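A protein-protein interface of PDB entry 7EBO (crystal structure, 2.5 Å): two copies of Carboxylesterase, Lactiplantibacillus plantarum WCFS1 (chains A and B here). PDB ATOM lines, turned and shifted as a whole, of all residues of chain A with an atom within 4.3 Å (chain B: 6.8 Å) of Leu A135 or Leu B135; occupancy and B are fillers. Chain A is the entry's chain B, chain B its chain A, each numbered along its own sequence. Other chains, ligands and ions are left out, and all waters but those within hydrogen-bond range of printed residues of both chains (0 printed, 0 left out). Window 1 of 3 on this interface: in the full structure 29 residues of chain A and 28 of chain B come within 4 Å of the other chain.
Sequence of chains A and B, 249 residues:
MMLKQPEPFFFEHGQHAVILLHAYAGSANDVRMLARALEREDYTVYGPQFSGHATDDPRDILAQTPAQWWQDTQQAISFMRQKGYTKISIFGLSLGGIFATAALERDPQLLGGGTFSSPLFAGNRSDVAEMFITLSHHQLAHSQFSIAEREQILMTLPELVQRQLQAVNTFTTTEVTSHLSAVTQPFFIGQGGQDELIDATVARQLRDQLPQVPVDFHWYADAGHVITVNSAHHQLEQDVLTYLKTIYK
Of the printed residues of chain B, Leu A135 touches Leu B135 (3.5 Å), His B138 (3.4 Å) and Gln B139 (3.8 Å).
Of the printed residues of chain B, His A138 touches Gln B139.
Phe B132 touches none of the printed residues of chain A.
Leu B135 touches three residues of chain A.
Ser B136 touches none of the printed residues of chain A.
Printed residues of chain A within 4 Å of His B142: Gln A139 (3.95 Å).
Met A131 touches Leu B135, but with the chains exchanged Leu A135 does not touch Met B131 (7.9 Å).
Thr A134 touches Leu B135, but with the chains exchanged Leu A135 does not touch Thr B134 (5.3 Å).
Leu A135 touches His B138, but with the chains exchanged His A138 does not touch Leu B135 (6.0 Å).
His A138 touches Gln B139, but with the chains exchanged Gln A139 does not touch His B138 (6.6 Å).
Of the 8 pairs that touch across the chains among the printed residues, 1 has its exchanged pair printed and touching as well.
Met A131 touches Thr B134.
CE of Met A131 touches CA of Leu B135, 3.4 Å away.
CD2 of Leu B135 touches CG2 of Thr A134 (3.8 Å).
CD2 of Leu A135 touches CD2 of Leu B135, 3.5 Å away.
Leu A135 touches His B138 (CD2 to CB, 3.4 Å).
CD2 of Leu A135 touches N of Gln B139, at 3.8 Å.
His A138 touches Gln B139 (CD2 to CB, 3.5 Å).
CD of Gln A139 touches NE2 of His B142 (3.95 Å).
The side-chain hydroxyl of Thr B134 lies within hydrogen-bond range of the backbone carbonyl oxygen of Glu B130 (3.2 Å).
The backbone carbonyl oxygen (O) of His B138 sits close to a ring nitrogen (ND1) of His B142, at 3.2 Å.
ND1 of His B142 sits at hydrogen-bond distance from O of Gln B139, at 3.5 Å.
Of the 9 printed residues of chain A, 5 touch a printed residue of chain B.
Hydrophobic or aromatic side chains of chain B within 4 Å of the printed part of chain A: Leu B135, His B138 and His B142.
Among the printed residues, no Asp or Glu carboxylate lies within 4 Å of a Lys or Arg side-chain nitrogen of the other chain.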
ATOM      1  N   MET A 131     -23.254  11.110  23.954  1.00  0.00           N
ATOM      2  CA  MET A 131     -24.548  11.028  24.621  1.00  0.00           C
ATOM      3  C   MET A 131     -25.670  10.807  23.614  1.00  0.00           C
ATOM      4  O   MET A 131     -26.559   9.975  23.829  1.00  0.00           O
ATOM      5  CB  MET A 131     -24.789  12.305  25.425  1.00  0.00           C
ATOM      6  CG  MET A 131     -26.054  12.285  26.248  1.00  0.00           C
ATOM      7  SD  MET A 131     -25.995  11.014  27.519  1.00  0.00           S
ATOM      8  CE  MET A 131     -27.718  10.552  27.553  1.00  0.00           C
ATOM      9  N   PHE A 132     -25.639  11.544  22.501  1.00  0.00           N
ATOM     10  CA  PHE A 132     -26.649  11.374  21.460  1.00  0.00           C
ATOM     11  C   PHE A 132     -26.567   9.992  20.825  1.00  0.00           C
ATOM     12  O   PHE A 132     -27.597   9.362  20.552  1.00  0.00           O
ATOM     13  CB  PHE A 132     -26.480  12.460  20.393  1.00  0.00           C
ATOM     14  CG  PHE A 132     -27.343  12.255  19.177  1.00  0.00           C
ATOM     15  CD1 PHE A 132     -28.583  12.859  19.070  1.00  0.00           C
ATOM     16  CD2 PHE A 132     -26.907  11.455  18.135  1.00  0.00           C
ATOM     17  CE1 PHE A 132     -29.369  12.664  17.947  1.00  0.00           C
ATOM     18  CE2 PHE A 132     -27.685  11.251  17.016  1.00  0.00           C
ATOM     19  CZ  PHE A 132     -28.914  11.858  16.916  1.00  0.00           C
ATOM     20  N   ILE A 133     -25.349   9.512  20.571  1.00  0.00           N
ATOM     21  CA  ILE A 133     -25.168   8.222  19.912  1.00  0.00           C
ATOM     22  C   ILE A 133     -25.691   7.091  20.789  1.00  0.00           C
ATOM     23  O   ILE A 133     -26.392   6.189  20.317  1.00  0.00           O
ATOM     24  CB  ILE A 133     -23.689   8.021  19.536  1.00  0.00           C
ATOM     25  CG1 ILE A 133     -23.297   8.981  18.407  1.00  0.00           C
ATOM     26  CG2 ILE A 133     -23.425   6.583  19.132  1.00  0.00           C
ATOM     27  CD1 ILE A 133     -21.808   9.071  18.169  1.00  0.00           C
ATOM     28  N   THR A 134     -25.355   7.120  22.080  1.00  0.00           N
ATOM     29  CA  THR A 134     -25.850   6.098  23.000  1.00  0.00           C
ATOM     30  C   THR A 134     -27.372   6.116  23.071  1.00  0.00           C
ATOM     31  O   THR A 134     -28.013   5.059  23.107  1.00  0.00           O
ATOM     32  CB  THR A 134     -25.241   6.303  24.389  1.00  0.00           C
ATOM     33  OG1 THR A 134     -23.815   6.241  24.292  1.00  0.00           O
ATOM     34  CG2 THR A 134     -25.717   5.227  25.347  1.00  0.00           C
ATOM     35  N   LEU A 135     -27.967   7.311  23.101  1.00  0.00           N
ATOM     36  CA  LEU A 135     -29.422   7.428  23.115  1.00  0.00           C
ATOM     37  C   LEU A 135     -30.031   6.861  21.841  1.00  0.00           C
ATOM     38  O   LEU A 135     -31.008   6.105  21.886  1.00  0.00           O
ATOM     39  CB  LEU A 135     -29.824   8.891  23.283  1.00  0.00           C
ATOM     40  CG  LEU A 135     -29.683   9.445  24.690  1.00  0.00           C
ATOM     41  CD1 LEU A 135     -30.087  10.914  24.723  1.00  0.00           C
ATOM     42  CD2 LEU A 135     -30.534   8.601  25.616  1.00  0.00           C
ATOM     43  N   SER A 136     -29.475   7.244  20.688  1.00  0.00           N
ATOM     44  CA  SER A 136     -30.000   6.774  19.411  1.00  0.00           C
ATOM     45  C   SER A 136     -29.916   5.257  19.320  1.00  0.00           C
ATOM     46  O   SER A 136     -30.845   4.603  18.831  1.00  0.00           O
ATOM     47  CB  SER A 136     -29.246   7.441  18.261  1.00  0.00           C
ATOM     48  OG  SER A 136     -29.225   8.853  18.416  1.00  0.00           O
ATOM     49  N   HIS A 137     -28.798   4.681  19.769  1.00  0.00           N
ATOM     50  CA  HIS A 137     -28.682   3.228  19.830  1.00  0.00           C
ATOM     51  C   HIS A 137     -29.829   2.626  20.630  1.00  0.00           C
ATOM     52  O   HIS A 137     -30.368   1.574  20.268  1.00  0.00           O
ATOM     53  CB  HIS A 137     -27.340   2.834  20.447  1.00  0.00           C
ATOM     54  CG  HIS A 137     -26.160   3.148  19.583  1.00  0.00           C
ATOM     55  ND1 HIS A 137     -24.869   2.842  19.954  1.00  0.00           N
ATOM     56  CD2 HIS A 137     -26.072   3.736  18.366  1.00  0.00           C
ATOM     57  CE1 HIS A 137     -24.036   3.226  19.003  1.00  0.00           C
ATOM     58  NE2 HIS A 137     -24.740   3.774  18.030  1.00  0.00           N
ATOM     59  N   HIS A 138     -30.208   3.279  21.732  1.00  0.00           N
ATOM     60  CA  HIS A 138     -31.317   2.791  22.544  1.00  0.00           C
ATOM     61  C   HIS A 138     -32.653   2.925  21.818  1.00  0.00           C
ATOM     62  O   HIS A 138     -33.501   2.029  21.913  1.00  0.00           O
ATOM     63  CB  HIS A 138     -31.353   3.525  23.882  1.00  0.00           C
ATOM     64  CG  HIS A 138     -32.402   3.016  24.817  1.00  0.00           C
ATOM     65  ND1 HIS A 138     -32.274   1.828  25.504  1.00  0.00           N
ATOM     66  CD2 HIS A 138     -33.604   3.528  25.174  1.00  0.00           C
ATOM     67  CE1 HIS A 138     -33.349   1.633  26.247  1.00  0.00           C
ATOM     68  NE2 HIS A 138     -34.171   2.651  26.065  1.00  0.00           N
ATOM     69  N   GLN A 139     -32.876   4.036  21.106  1.00  0.00           N
ATOM     70  CA  GLN A 139     -34.112   4.157  20.334  1.00  0.00           C
ATOM     71  C   GLN A 139     -34.190   3.079  19.264  1.00  0.00           C
ATOM     72  O   GLN A 139     -35.225   2.424  19.093  1.00  0.00           O
ATOM     73  CB  GLN A 139     -34.214   5.518  19.639  1.00  0.00           C
ATOM     74  CG  GLN A 139     -34.383   6.768  20.463  1.00  0.00           C
ATOM     75  CD  GLN A 139     -34.579   7.978  19.561  1.00  0.00           C
ATOM     76  OE1 GLN A 139     -35.570   8.059  18.822  1.00  0.00           O
ATOM     77  NE2 GLN A 139     -33.642   8.906  19.600  1.00  0.00           N
ATOM     78  N   TYR B  24     -20.449   0.446  30.690  1.00  0.00           N
ATOM     79  CA  TYR B  24     -21.487   0.415  31.715  1.00  0.00           C
ATOM     80  C   TYR B  24     -22.735   1.137  31.220  1.00  0.00           C
ATOM     81  O   TYR B  24     -22.654   2.257  30.704  1.00  0.00           O
ATOM     82  CB  TYR B  24     -20.957   1.061  32.996  1.00  0.00           C
ATOM     83  CG  TYR B  24     -21.920   1.089  34.161  1.00  0.00           C
ATOM     84  CD1 TYR B  24     -22.311  -0.083  34.799  1.00  0.00           C
ATOM     85  CD2 TYR B  24     -22.421   2.291  34.639  1.00  0.00           C
ATOM     86  CE1 TYR B  24     -23.183  -0.056  35.874  1.00  0.00           C
ATOM     87  CE2 TYR B  24     -23.293   2.328  35.711  1.00  0.00           C
ATOM     88  CZ  TYR B  24     -23.672   1.154  36.325  1.00  0.00           C
ATOM     89  OH  TYR B  24     -24.541   1.194  37.394  1.00  0.00           O
ATOM     90  N   ALA B  25     -23.888   0.478  31.356  1.00  0.00           N
ATOM     91  CA  ALA B  25     -25.184   0.972  30.886  1.00  0.00           C
ATOM     92  C   ALA B  25     -25.225   1.145  29.370  1.00  0.00           C
ATOM     93  O   ALA B  25     -26.113   1.826  28.847  1.00  0.00           O
ATOM     94  CB  ALA B  25     -25.583   2.282  31.575  1.00  0.00           C
ATOM     95  N   GLY B  26     -24.277   0.550  28.659  1.00  0.00           N
ATOM     96  CA  GLY B  26     -24.248   0.532  27.210  1.00  0.00           C
ATOM     97  C   GLY B  26     -24.806  -0.755  26.642  1.00  0.00           C
ATOM     98  O   GLY B  26     -25.672  -1.404  27.242  1.00  0.00           O
ATOM     99  N   PRO B  58     -33.614   0.422  33.383  1.00  0.00           N
ATOM    100  CA  PRO B  58     -32.268   0.644  33.935  1.00  0.00           C
ATOM    101  C   PRO B  58     -32.025  -0.108  35.233  1.00  0.00           C
ATOM    102  O   PRO B  58     -30.863  -0.369  35.575  1.00  0.00           O
ATOM    103  CB  PRO B  58     -32.225   2.161  34.157  1.00  0.00           C
ATOM    104  CG  PRO B  58     -33.253   2.709  33.216  1.00  0.00           C
ATOM    105  CD  PRO B  58     -34.349   1.684  33.203  1.00  0.00           C
ATOM    106  N   ILE B  61     -29.880  -3.355  35.170  1.00  0.00           N
ATOM    107  CA  ILE B  61     -28.436  -3.240  35.338  1.00  0.00           C
ATOM    108  C   ILE B  61     -28.073  -3.254  36.816  1.00  0.00           C
ATOM    109  O   ILE B  61     -27.122  -3.925  37.232  1.00  0.00           O
ATOM    110  CB  ILE B  61     -27.930  -1.960  34.648  1.00  0.00           C
ATOM    111  CG1 ILE B  61     -28.205  -2.005  33.144  1.00  0.00           C
ATOM    112  CG2 ILE B  61     -26.450  -1.756  34.916  1.00  0.00           C
ATOM    113  CD1 ILE B  61     -28.181  -0.637  32.486  1.00  0.00           C
ATOM    114  N   GLU B 130     -23.627  10.308  37.284  1.00  0.00           N
ATOM    115  CA  GLU B 130     -24.499  11.343  36.741  1.00  0.00           C
ATOM    116  C   GLU B 130     -24.821  11.096  35.274  1.00  0.00           C
ATOM    117  O   GLU B 130     -25.925  11.420  34.820  1.00  0.00           O
ATOM    118  CB  GLU B 130     -23.861  12.714  36.934  1.00  0.00           C
ATOM    119  CG  GLU B 130     -23.743  13.135  38.382  1.00  0.00           C
ATOM    120  CD  GLU B 130     -25.097  13.355  39.024  1.00  0.00           C
ATOM    121  OE1 GLU B 130     -26.077  13.609  38.289  1.00  0.00           O
ATOM    122  OE2 GLU B 130     -25.187  13.271  40.266  1.00  0.00           O
ATOM    123  N   MET B 131     -23.872  10.537  34.521  1.00  0.00           N
ATOM    124  CA  MET B 131     -24.142  10.186  33.131  1.00  0.00           C
ATOM    125  C   MET B 131     -25.256   9.153  33.041  1.00  0.00           C
ATOM    126  O   MET B 131     -26.114   9.225  32.154  1.00  0.00           O
ATOM    127  CB  MET B 131     -22.869   9.665  32.465  1.00  0.00           C
ATOM    128  N   PHE B 132     -25.248   8.177  33.952  1.00  0.00           N
ATOM    129  CA  PHE B 132     -26.273   7.141  33.956  1.00  0.00           C
ATOM    130  C   PHE B 132     -27.650   7.746  34.202  1.00  0.00           C
ATOM    131  O   PHE B 132     -28.641   7.318  33.599  1.00  0.00           O
ATOM    132  CB  PHE B 132     -25.925   6.093  35.018  1.00  0.00           C
ATOM    133  CG  PHE B 132     -26.938   4.991  35.158  1.00  0.00           C
ATOM    134  CD1 PHE B 132     -26.795   3.823  34.430  1.00  0.00           C
ATOM    135  CD2 PHE B 132     -28.008   5.100  36.026  1.00  0.00           C
ATOM    136  CE1 PHE B 132     -27.706   2.791  34.552  1.00  0.00           C
ATOM    137  CE2 PHE B 132     -28.923   4.069  36.154  1.00  0.00           C
ATOM    138  CZ  PHE B 132     -28.772   2.914  35.415  1.00  0.00           C
ATOM    139  N   ILE B 133     -27.733   8.734  35.097  1.00  0.00           N
ATOM    140  CA  ILE B 133     -29.008   9.391  35.374  1.00  0.00           C
ATOM    141  C   ILE B 133     -29.493  10.148  34.141  1.00  0.00           C
ATOM    142  O   ILE B 133     -30.662  10.046  33.748  1.00  0.00           O
ATOM    143  CB  ILE B 133     -28.875  10.324  36.591  1.00  0.00           C
ATOM    144  CG1 ILE B 133     -28.688   9.513  37.877  1.00  0.00           C
ATOM    145  CG2 ILE B 133     -30.091  11.228  36.702  1.00  0.00           C
ATOM    146  CD1 ILE B 133     -28.246  10.349  39.059  1.00  0.00           C
ATOM    147  N   THR B 134     -28.598  10.917  33.514  1.00  0.00           N
ATOM    148  CA  THR B 134     -28.944  11.616  32.280  1.00  0.00           C
ATOM    149  C   THR B 134     -29.333  10.632  31.187  1.00  0.00           C
ATOM    150  O   THR B 134     -30.300  10.854  30.448  1.00  0.00           O
ATOM    151  CB  THR B 134     -27.763  12.472  31.821  1.00  0.00           C
ATOM    152  OG1 THR B 134     -27.448  13.451  32.820  1.00  0.00           O
ATOM    153  CG2 THR B 134     -28.048  13.144  30.484  1.00  0.00           C
ATOM    154  N   LEU B 135     -28.587   9.532  31.078  1.00  0.00           N
ATOM    155  CA  LEU B 135     -28.880   8.514  30.078  1.00  0.00           C
ATOM    156  C   LEU B 135     -30.243   7.877  30.324  1.00  0.00           C
ATOM    157  O   LEU B 135     -31.064   7.767  29.409  1.00  0.00           O
ATOM    158  CB  LEU B 135     -27.767   7.466  30.099  1.00  0.00           C
ATOM    159  CG  LEU B 135     -27.426   6.569  28.906  1.00  0.00           C
ATOM    160  CD1 LEU B 135     -27.664   5.113  29.271  1.00  0.00           C
ATOM    161  CD2 LEU B 135     -28.197   6.953  27.660  1.00  0.00           C
ATOM    162  N   SER B 136     -30.502   7.465  31.566  1.00  0.00           N
ATOM    163  CA  SER B 136     -31.754   6.783  31.884  1.00  0.00           C
ATOM    164  C   SER B 136     -32.966   7.682  31.652  1.00  0.00           C
ATOM    165  O   SER B 136     -33.972   7.246  31.080  1.00  0.00           O
ATOM    166  CB  SER B 136     -31.719   6.290  33.331  1.00  0.00           C
ATOM    167  OG  SER B 136     -30.546   5.538  33.585  1.00  0.00           O
ATOM    168  N   HIS B 137     -32.901   8.934  32.117  1.00  0.00           N
ATOM    169  CA  HIS B 137     -34.007   9.868  31.905  1.00  0.00           C
ATOM    170  C   HIS B 137     -34.328  10.038  30.427  1.00  0.00           C
ATOM    171  O   HIS B 137     -35.500  10.047  30.033  1.00  0.00           O
ATOM    172  CB  HIS B 137     -33.683  11.228  32.521  1.00  0.00           C
ATOM    173  CG  HIS B 137     -34.436  12.362  31.894  1.00  0.00           C
ATOM    174  ND1 HIS B 137     -35.778  12.580  32.122  1.00  0.00           N
ATOM    175  CD2 HIS B 137     -34.038  13.328  31.033  1.00  0.00           C
ATOM    176  CE1 HIS B 137     -36.172  13.639  31.436  1.00  0.00           C
ATOM    177  NE2 HIS B 137     -35.135  14.111  30.767  1.00  0.00           N
ATOM    178  N   HIS B 138     -33.299  10.186  29.595  1.00  0.00           N
ATOM    179  CA  HIS B 138     -33.530  10.335  28.164  1.00  0.00           C
ATOM    180  C   HIS B 138     -34.026   9.032  27.541  1.00  0.00           C
ATOM    181  O   HIS B 138     -34.891   9.057  26.658  1.00  0.00           O
ATOM    182  CB  HIS B 138     -32.262  10.839  27.481  1.00  0.00           C
ATOM    183  CG  HIS B 138     -32.065  12.320  27.587  1.00  0.00           C
ATOM    184  ND1 HIS B 138     -33.054  13.226  27.270  1.00  0.00           N
ATOM    185  CD2 HIS B 138     -30.990  13.053  27.963  1.00  0.00           C
ATOM    186  CE1 HIS B 138     -32.599  14.453  27.451  1.00  0.00           C
ATOM    187  NE2 HIS B 138     -31.349  14.376  27.872  1.00  0.00           N
ATOM    188  N   GLN B 139     -33.480   7.887  27.969  1.00  0.00           N
ATOM    189  CA  GLN B 139     -33.970   6.607  27.463  1.00  0.00           C
ATOM    190  C   GLN B 139     -35.435   6.400  27.826  1.00  0.00           C
ATOM    191  O   GLN B 139     -36.226   5.918  27.008  1.00  0.00           O
ATOM    192  CB  GLN B 139     -33.134   5.448  28.011  1.00  0.00           C
ATOM    193  CG  GLN B 139     -31.702   5.379  27.516  1.00  0.00           C
ATOM    194  CD  GLN B 139     -30.981   4.142  28.018  1.00  0.00           C
ATOM    195  OE1 GLN B 139     -31.398   3.522  28.999  1.00  0.00           O
ATOM    196  NE2 GLN B 139     -29.905   3.767  27.340  1.00  0.00           N
ATOM    197  N   LEU B 140     -35.807   6.746  29.059  1.00  0.00           N
ATOM    198  CA  LEU B 140     -37.173   6.553  29.531  1.00  0.00           C
ATOM    199  C   LEU B 140     -38.182   7.404  28.772  1.00  0.00           C
ATOM    200  O   LEU B 140     -39.375   7.081  28.781  1.00  0.00           O
ATOM    201  CB  LEU B 140     -37.257   6.839  31.029  1.00  0.00           C
ATOM    202  CG  LEU B 140     -36.687   5.720  31.909  1.00  0.00           C
ATOM    203  CD1 LEU B 140     -36.429   6.198  33.333  1.00  0.00           C
ATOM    204  CD2 LEU B 140     -37.608   4.509  31.903  1.00  0.00           C
ATOM    205  N   HIS B 142     -38.761   7.490  25.789  1.00  0.00           N
ATOM    206  CA  HIS B 142     -39.363   6.618  24.791  1.00  0.00           C
ATOM    207  C   HIS B 142     -39.788   5.286  25.392  1.00  0.00           C
ATOM    208  O   HIS B 142     -40.104   4.349  24.650  1.00  0.00           O
ATOM    209  CB  HIS B 142     -38.390   6.391  23.636  1.00  0.00           C
ATOM    210  CG  HIS B 142     -37.511   7.570  23.364  1.00  0.00           C
ATOM    211  ND1 HIS B 142     -36.351   7.808  24.069  1.00  0.00           N
ATOM    212  CD2 HIS B 142     -37.634   8.592  22.486  1.00  0.00           C
ATOM    213  CE1 HIS B 142     -35.791   8.919  23.627  1.00  0.00           C
ATOM    214  NE2 HIS B 142     -36.551   9.416  22.668  1.00  0.00           N
